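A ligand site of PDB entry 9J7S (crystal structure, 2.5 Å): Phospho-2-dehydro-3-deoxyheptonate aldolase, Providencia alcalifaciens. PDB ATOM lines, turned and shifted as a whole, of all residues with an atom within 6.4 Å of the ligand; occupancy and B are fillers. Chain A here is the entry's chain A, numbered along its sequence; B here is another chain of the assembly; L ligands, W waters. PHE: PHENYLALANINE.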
ATOM      1  N   ARG A  40       2.734 -21.919  28.701  1.00  0.00           N
ATOM      2  CA  ARG A  40       2.258 -21.020  27.659  1.00  0.00           C
ATOM      3  C   ARG A  40       1.251 -19.984  28.189  1.00  0.00           C
ATOM      4  O   ARG A  40       1.284 -18.824  27.755  1.00  0.00           O
ATOM      5  CB  ARG A  40       1.554 -21.756  26.518  1.00  0.00           C
ATOM      6  CG  ARG A  40       2.445 -22.620  25.632  1.00  0.00           C
ATOM      7  CD  ARG A  40       1.547 -23.472  24.753  1.00  0.00           C
ATOM      8  NE  ARG A  40       2.348 -24.202  23.775  1.00  0.00           N
ATOM      9  CZ  ARG A  40       1.878 -25.071  22.893  1.00  0.00           C
ATOM     10  NH1 ARG A  40       0.599 -25.310  22.790  1.00  0.00           N
ATOM     11  NH2 ARG A  40       2.706 -25.718  22.096  1.00  0.00           N
ATOM     12  N   VAL A 147       9.475 -23.815   8.469  1.00  0.00           N
ATOM     13  CA  VAL A 147       8.050 -24.058   8.600  1.00  0.00           C
ATOM     14  C   VAL A 147       7.687 -25.543   8.682  1.00  0.00           C
ATOM     15  O   VAL A 147       6.541 -25.871   8.673  1.00  0.00           O
ATOM     16  CB  VAL A 147       7.291 -23.454   7.396  1.00  0.00           C
ATOM     17  CG1 VAL A 147       7.751 -22.029   7.152  1.00  0.00           C
ATOM     18  CG2 VAL A 147       7.423 -24.321   6.139  1.00  0.00           C
ATOM     19  N   ILE A 148       8.649 -26.458   8.663  1.00  0.00           N
ATOM     20  CA  ILE A 148       8.342 -27.881   8.666  1.00  0.00           C
ATOM     21  C   ILE A 148       8.666 -28.527  10.017  1.00  0.00           C
ATOM     22  O   ILE A 148       7.905 -29.381  10.479  1.00  0.00           O
ATOM     23  CB  ILE A 148       9.076 -28.586   7.503  1.00  0.00           C
ATOM     24  CG1 ILE A 148       8.531 -28.062   6.194  1.00  0.00           C
ATOM     25  CG2 ILE A 148       8.979 -30.112   7.597  1.00  0.00           C
ATOM     26  CD1 ILE A 148       8.993 -28.822   4.985  1.00  0.00           C
ATOM     27  N   PRO A 150       8.551 -27.382  13.085  1.00  0.00           N
ATOM     28  CA  PRO A 150       7.565 -27.264  14.150  1.00  0.00           C
ATOM     29  C   PRO A 150       6.561 -28.410  14.235  1.00  0.00           C
ATOM     30  O   PRO A 150       6.027 -28.701  15.312  1.00  0.00           O
ATOM     31  CB  PRO A 150       6.894 -25.956  13.817  1.00  0.00           C
ATOM     32  CG  PRO A 150       7.967 -25.172  13.143  1.00  0.00           C
ATOM     33  CD  PRO A 150       8.600 -26.197  12.198  1.00  0.00           C
ATOM     34  N   GLN A 151       6.274 -29.078  13.113  1.00  0.00           N
ATOM     35  CA  GLN A 151       5.265 -30.125  13.162  1.00  0.00           C
ATOM     36  C   GLN A 151       5.750 -31.300  14.001  1.00  0.00           C
ATOM     37  O   GLN A 151       4.934 -32.097  14.446  1.00  0.00           O
ATOM     38  CB  GLN A 151       4.835 -30.504  11.751  1.00  0.00           C
ATOM     39  CG  GLN A 151       3.900 -29.449  11.143  1.00  0.00           C
ATOM     40  CD  GLN A 151       2.477 -29.580  11.628  1.00  0.00           C
ATOM     41  OE1 GLN A 151       2.184 -29.481  12.838  1.00  0.00           O
ATOM     42  NE2 GLN A 151       1.562 -29.862  10.702  1.00  0.00           N
ATOM     43  N   ALA A 154       6.611 -28.780  18.193  1.00  0.00           N
ATOM     44  CA  ALA A 154       5.987 -27.579  18.735  1.00  0.00           C
ATOM     45  C   ALA A 154       5.030 -27.905  19.880  1.00  0.00           C
ATOM     46  O   ALA A 154       4.818 -27.049  20.758  1.00  0.00           O
ATOM     47  CB  ALA A 154       5.250 -26.851  17.635  1.00  0.00           C
ATOM     48  N   ASP A 155       4.428 -29.112  19.845  1.00  0.00           N
ATOM     49  CA  ASP A 155       3.513 -29.521  20.882  1.00  0.00           C
ATOM     50  C   ASP A 155       4.233 -29.635  22.249  1.00  0.00           C
ATOM     51  O   ASP A 155       3.570 -29.666  23.284  1.00  0.00           O
ATOM     52  CB  ASP A 155       2.777 -30.772  20.465  1.00  0.00           C
ATOM     53  CG  ASP A 155       3.649 -32.012  20.363  1.00  0.00           C
ATOM     54  OD1 ASP A 155       4.554 -31.993  19.513  1.00  0.00           O
ATOM     55  OD2 ASP A 155       3.434 -32.959  21.149  1.00  0.00           O
ATOM     56  N   LEU A 175       4.541 -17.974   9.914  1.00  0.00           N
ATOM     57  CA  LEU A 175       4.646 -19.145  10.781  1.00  0.00           C
ATOM     58  C   LEU A 175       4.269 -18.746  12.209  1.00  0.00           C
ATOM     59  O   LEU A 175       3.493 -19.415  12.879  1.00  0.00           O
ATOM     60  CB  LEU A 175       6.072 -19.712  10.712  1.00  0.00           C
ATOM     61  CG  LEU A 175       6.362 -20.856  11.693  1.00  0.00           C
ATOM     62  CD1 LEU A 175       5.598 -22.166  11.400  1.00  0.00           C
ATOM     63  CD2 LEU A 175       7.850 -21.067  11.817  1.00  0.00           C
ATOM     64  N   GLY A 178       0.722 -18.730  13.184  1.00  0.00           N
ATOM     65  CA  GLY A 178       0.004 -19.976  13.396  1.00  0.00           C
ATOM     66  C   GLY A 178       0.634 -20.896  14.458  1.00  0.00           C
ATOM     67  O   GLY A 178       0.273 -22.097  14.528  1.00  0.00           O
ATOM     68  N   LEU A 179       1.547 -20.373  15.278  1.00  0.00           N
ATOM     69  CA  LEU A 179       2.182 -21.232  16.281  1.00  0.00           C
ATOM     70  C   LEU A 179       1.357 -21.223  17.551  1.00  0.00           C
ATOM     71  O   LEU A 179       0.831 -20.175  17.916  1.00  0.00           O
ATOM     72  CB  LEU A 179       3.625 -20.843  16.615  1.00  0.00           C
ATOM     73  CG  LEU A 179       4.699 -21.217  15.575  1.00  0.00           C
ATOM     74  CD1 LEU A 179       5.944 -20.472  15.961  1.00  0.00           C
ATOM     75  CD2 LEU A 179       4.922 -22.705  15.505  1.00  0.00           C
ATOM     76  N   SER A 180       1.328 -22.376  18.255  1.00  0.00           N
ATOM     77  CA  SER A 180       0.562 -22.503  19.496  1.00  0.00           C
ATOM     78  C   SER A 180       1.187 -21.758  20.685  1.00  0.00           C
ATOM     79  O   SER A 180       0.560 -21.640  21.728  1.00  0.00           O
ATOM     80  CB  SER A 180       0.333 -23.930  19.851  1.00  0.00           C
ATOM     81  OG  SER A 180      -0.207 -24.652  18.775  1.00  0.00           O
ATOM     82  N   CYS A 181       2.430 -21.297  20.591  1.00  0.00           N
ATOM     83  CA  CYS A 181       3.067 -20.710  21.753  1.00  0.00           C
ATOM     84  C   CYS A 181       3.335 -19.235  21.499  1.00  0.00           C
ATOM     85  O   CYS A 181       3.118 -18.754  20.402  1.00  0.00           O
ATOM     86  CB  CYS A 181       4.361 -21.461  22.109  1.00  0.00           C
ATOM     87  SG  CYS A 181       5.522 -21.499  20.728  1.00  0.00           S
ATOM     88  N   PHE A 209       0.452 -20.318   4.613  1.00  0.00           N
ATOM     89  CA  PHE A 209       1.844 -20.747   4.330  1.00  0.00           C
ATOM     90  C   PHE A 209       1.809 -22.227   3.954  1.00  0.00           C
ATOM     91  O   PHE A 209       0.905 -22.973   4.303  1.00  0.00           O
ATOM     92  CB  PHE A 209       2.808 -20.410   5.471  1.00  0.00           C
ATOM     93  CG  PHE A 209       2.680 -21.161   6.794  1.00  0.00           C
ATOM     94  CD1 PHE A 209       1.939 -20.626   7.838  1.00  0.00           C
ATOM     95  CD2 PHE A 209       3.344 -22.364   6.998  1.00  0.00           C
ATOM     96  CE1 PHE A 209       1.858 -21.288   9.049  1.00  0.00           C
ATOM     97  CE2 PHE A 209       3.249 -23.024   8.208  1.00  0.00           C
ATOM     98  CZ  PHE A 209       2.501 -22.491   9.230  1.00  0.00           C
ATOM     99  N   SER A 211       3.414 -25.990   4.200  1.00  0.00           N
ATOM    100  CA  SER A 211       4.239 -26.919   4.995  1.00  0.00           C
ATOM    101  C   SER A 211       3.424 -28.218   4.942  1.00  0.00           C
ATOM    102  O   SER A 211       2.516 -28.333   4.120  1.00  0.00           O
ATOM    103  CB  SER A 211       4.292 -26.607   6.444  1.00  0.00           C
ATOM    104  OG  SER A 211       5.181 -27.479   7.139  1.00  0.00           O
ATOM    105  N   VAL A 212       3.776 -29.131   5.811  1.00  0.00           N
ATOM    106  CA  VAL A 212       3.148 -30.470   5.760  1.00  0.00           C
ATOM    107  C   VAL A 212       2.140 -30.764   6.857  1.00  0.00           C
ATOM    108  O   VAL A 212       2.096 -30.039   7.865  1.00  0.00           O
ATOM    109  CB  VAL A 212       4.364 -31.435   5.817  1.00  0.00           C
ATOM    110  CG1 VAL A 212       5.216 -31.405   4.564  1.00  0.00           C
ATOM    111  CG2 VAL A 212       5.202 -31.236   7.076  1.00  0.00           C
ATOM    112  N   THR A 213       1.340 -31.781   6.641  1.00  0.00           N
ATOM    113  CA  THR A 213       0.403 -32.241   7.656  1.00  0.00           C
ATOM    114  C   THR A 213       1.141 -33.131   8.629  1.00  0.00           C
ATOM    115  O   THR A 213       2.303 -33.469   8.358  1.00  0.00           O
ATOM    116  CB  THR A 213      -0.694 -33.000   6.910  1.00  0.00           C
ATOM    117  OG1 THR A 213      -0.029 -34.095   6.304  1.00  0.00           O
ATOM    118  CG2 THR A 213      -1.384 -32.138   5.877  1.00  0.00           C
ATOM    119  N   LYS A 214       0.527 -33.464   9.753  1.00  0.00           N
ATOM    120  CA  LYS A 214       1.091 -34.437  10.657  1.00  0.00           C
ATOM    121  C   LYS A 214       1.453 -35.718   9.908  1.00  0.00           C
ATOM    122  O   LYS A 214       2.348 -36.435  10.338  1.00  0.00           O
ATOM    123  CB  LYS A 214       0.122 -34.737  11.827  1.00  0.00           C
ATOM    124  CG  LYS A 214      -0.112 -33.625  12.824  1.00  0.00           C
ATOM    125  CD  LYS A 214       1.181 -32.940  13.205  1.00  0.00           C
ATOM    126  CE  LYS A 214       1.144 -32.149  14.468  1.00  0.00           C
ATOM    127  NZ  LYS A 214       0.491 -30.853  14.351  1.00  0.00           N
ATOM    128  N   VAL A 221      -1.561 -24.188   5.186  1.00  0.00           N
ATOM    129  CA  VAL A 221      -1.838 -23.932   6.587  1.00  0.00           C
ATOM    130  C   VAL A 221      -2.435 -22.547   6.652  1.00  0.00           C
ATOM    131  O   VAL A 221      -1.742 -21.597   6.282  1.00  0.00           O
ATOM    132  CB  VAL A 221      -0.612 -24.046   7.520  1.00  0.00           C
ATOM    133  CG1 VAL A 221      -0.967 -24.002   8.994  1.00  0.00           C
ATOM    134  CG2 VAL A 221       0.144 -25.328   7.280  1.00  0.00           C
ATOM    135  N   ASN B   5      -2.843 -28.909  23.074  1.00  0.00           N
ATOM    136  CA  ASN B   5      -1.640 -28.091  22.855  1.00  0.00           C
ATOM    137  C   ASN B   5      -1.319 -27.948  21.361  1.00  0.00           C
ATOM    138  O   ASN B   5      -0.539 -27.087  20.963  1.00  0.00           O
ATOM    139  CB  ASN B   5      -0.414 -28.622  23.593  1.00  0.00           C
ATOM    140  CG  ASN B   5      -0.573 -28.646  25.101  1.00  0.00           C
ATOM    141  OD1 ASN B   5      -0.026 -29.503  25.802  1.00  0.00           O
ATOM    142  ND2 ASN B   5      -1.290 -27.676  25.632  1.00  0.00           N
ATOM    143  N   ASP B   6      -1.964 -28.773  20.519  1.00  0.00           N
ATOM    144  CA  ASP B   6      -1.585 -28.870  19.132  1.00  0.00           C
ATOM    145  C   ASP B   6      -2.470 -27.970  18.283  1.00  0.00           C
ATOM    146  O   ASP B   6      -3.694 -28.039  18.349  1.00  0.00           O
ATOM    147  CB  ASP B   6      -1.605 -30.320  18.701  1.00  0.00           C
ATOM    148  CG  ASP B   6      -0.991 -30.553  17.339  1.00  0.00           C
ATOM    149  OD1 ASP B   6       0.090 -29.975  17.096  1.00  0.00           O
ATOM    150  OD2 ASP B   6      -1.589 -31.299  16.537  1.00  0.00           O
ATOM    151  N   ASP B   7      -1.842 -27.151  17.424  1.00  0.00           N
ATOM    152  CA  ASP B   7      -2.569 -26.492  16.356  1.00  0.00           C
ATOM    153  C   ASP B   7      -3.634 -25.542  16.926  1.00  0.00           C
ATOM    154  O   ASP B   7      -4.700 -25.375  16.324  1.00  0.00           O
ATOM    155  CB  ASP B   7      -3.227 -27.484  15.403  1.00  0.00           C
ATOM    156  CG  ASP B   7      -2.348 -28.108  14.324  1.00  0.00           C
ATOM    157  OD1 ASP B   7      -1.169 -27.777  14.248  1.00  0.00           O
ATOM    158  OD2 ASP B   7      -2.821 -28.959  13.568  1.00  0.00           O
ATOM    159  N   VAL B   8      -3.348 -24.873  18.062  1.00  0.00           N
ATOM    160  CA  VAL B   8      -4.404 -24.047  18.636  1.00  0.00           C
ATOM    161  C   VAL B   8      -4.608 -22.836  17.725  1.00  0.00           C
ATOM    162  O   VAL B   8      -5.690 -22.280  17.745  1.00  0.00           O
ATOM    163  CB  VAL B   8      -4.356 -23.617  20.118  1.00  0.00           C
ATOM    164  CG1 VAL B   8      -3.516 -24.567  20.995  1.00  0.00           C
ATOM    165  CG2 VAL B   8      -3.968 -22.164  20.341  1.00  0.00           C
ATOM    166  N   ARG B   9      -3.617 -22.436  16.921  1.00  0.00           N
ATOM    167  CA  ARG B   9      -3.796 -21.285  16.041  1.00  0.00           C
ATOM    168  C   ARG B   9      -3.756 -21.697  14.572  1.00  0.00           C
ATOM    169  O   ARG B   9      -3.495 -20.897  13.673  1.00  0.00           O
ATOM    170  CB  ARG B   9      -2.705 -20.245  16.244  1.00  0.00           C
ATOM    171  CG  ARG B   9      -2.738 -19.622  17.625  1.00  0.00           C
ATOM    172  CD  ARG B   9      -1.833 -18.406  17.635  1.00  0.00           C
ATOM    173  NE  ARG B   9      -2.025 -17.767  18.946  1.00  0.00           N
ATOM    174  CZ  ARG B   9      -1.438 -18.159  20.079  1.00  0.00           C
ATOM    175  NH1 ARG B   9      -0.344 -18.909  20.074  1.00  0.00           N
ATOM    176  NH2 ARG B   9      -1.892 -17.649  21.197  1.00  0.00           N
ATOM    177  N   VAL B  10      -4.123 -22.937  14.290  1.00  0.00           N
ATOM    178  CA  VAL B  10      -4.359 -23.303  12.902  1.00  0.00           C
ATOM    179  C   VAL B  10      -5.868 -23.345  12.701  1.00  0.00           C
ATOM    180  O   VAL B  10      -6.530 -24.117  13.346  1.00  0.00           O
ATOM    181  CB  VAL B  10      -3.651 -24.634  12.625  1.00  0.00           C
ATOM    182  CG1 VAL B  10      -3.947 -25.117  11.211  1.00  0.00           C
ATOM    183  CG2 VAL B  10      -2.143 -24.510  12.828  1.00  0.00           C
ATOM    184  N   ILE B  13      -5.939 -26.739   7.937  1.00  0.00           N
ATOM    185  CA  ILE B  13      -4.787 -27.298   7.262  1.00  0.00           C
ATOM    186  C   ILE B  13      -5.324 -28.344   6.290  1.00  0.00           C
ATOM    187  O   ILE B  13      -6.040 -29.240   6.723  1.00  0.00           O
ATOM    188  CB  ILE B  13      -3.792 -27.907   8.270  1.00  0.00           C
ATOM    189  CG1 ILE B  13      -2.578 -28.472   7.619  1.00  0.00           C
ATOM    190  CG2 ILE B  13      -4.429 -28.951   9.191  1.00  0.00           C
ATOM    191  CD1 ILE B  13      -1.446 -28.718   8.598  1.00  0.00           C
HETATM  192  N   PHE L   1       1.937 -27.388  14.885  1.00  0.00           N
HETATM  193  CA  PHE L   1       2.268 -25.942  15.065  1.00  0.00           C
HETATM  194  C   PHE L   1       1.838 -25.476  16.475  1.00  0.00           C
HETATM  195  O   PHE L   1       0.959 -26.219  16.940  1.00  0.00           O
HETATM  196  CB  PHE L   1       1.568 -25.174  13.931  1.00  0.00           C
HETATM  197  CG  PHE L   1       2.040 -25.592  12.550  1.00  0.00           C
HETATM  198  CD1 PHE L   1       1.245 -26.405  11.768  1.00  0.00           C
HETATM  199  CD2 PHE L   1       3.284 -25.225  12.084  1.00  0.00           C
HETATM  200  CE1 PHE L   1       1.671 -26.807  10.513  1.00  0.00           C
HETATM  201  CE2 PHE L   1       3.735 -25.649  10.847  1.00  0.00           C
HETATM  202  CZ  PHE L   1       2.926 -26.462  10.050  1.00  0.00           C
HETATM  203  OXT PHE L   1       2.244 -24.415  17.049  1.00  0.00           O
HETATM  204  O   HOH W   1      -1.193 -23.597  16.472  1.00  0.00           O
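N of Ser 180 lies within hydrogen-bond range of OXT of the ligand. O of the ligand sits at hydrogen-bond distance from OG of Ser 180 (2.7 Å). A nitrogen (N) of the ligand is in hydrogen-bond range of the side-chain amide oxygen (OE1) of Gln 151. The backbone NH of Asp 7 of chain B is in hydrogen-bond range of an oxygen (O) of the ligand (3.0 Å). The side-chain carboxylate of Asp 7 of chain B lies within salt-bridge range of a nitrogen (N) of the ligand, 3.2 Å away. A nitrogen (N) of the ligand lies within salt-bridge range of the side-chain carboxylate (OD1) of Asp 6 of chain B (3.9 Å).
OG of Ser 180 lies within hydrogen-bond range of N of Asp 7 of chain B, at 3.3 Å. O of Asn 5 of chain B sits at hydrogen-bond distance from OG of Ser 180 (3.3 Å). The side-chain hydroxyl (OG) of Ser 180 lies within hydrogen-bond range of the backbone NH (N) of Val 8 of chain B (3.2 Å). O of Ser 180 sits close to NH1 of Arg 9 of chain B (3.3 Å). O of Val 212 lies within hydrogen-bond range of NE2 of Gln 151, 2.9 Å away. The side-chain carboxylate (OD1) of Asp 7 of chain B is in salt-bridge range of the side-chain amino group (NZ) of Lys 214 (3.5 Å). The backbone carbonyl oxygen of Val 147 lies within hydrogen-bond range of the side-chain hydroxyl of Ser 211 (2.6 Å). NH2 of Arg 40 lies within hydrogen-bond range of O of Ala 154 (2.8 Å).
Merely in contact with the ligand: Val 147, Ala 154, Leu 175, Gly 178, Leu 179, Phe 209, Ser 211, Lys 214, Val 221 and Val 10 of chain B. Hydrophobic or aromatic side chains within 4 Å of the ligand: Ala 154, Leu 175, Leu 179, Phe 209, Val 221 and Val 10 of chain B. Within 4 Å of the ligand: Val 147, Gln 151, Ala 154, Leu 175, Gly 178, Leu 179, Ser 180, Phe 209, Ser 211, Lys 214, Val 221, Asp 6 of chain B, Asp 7 of chain B and Val 10 of chain B.
Water W1 lies within hydrogen-bond range of the side-chain hydroxyl (OG) of Ser 180, the backbone NH (N) of Arg 9 of chain B, the backbone carbonyl oxygen (O) of Gly 178, the backbone NH (N) of Val 8 of chain B and an oxygen (O) of the ligand.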
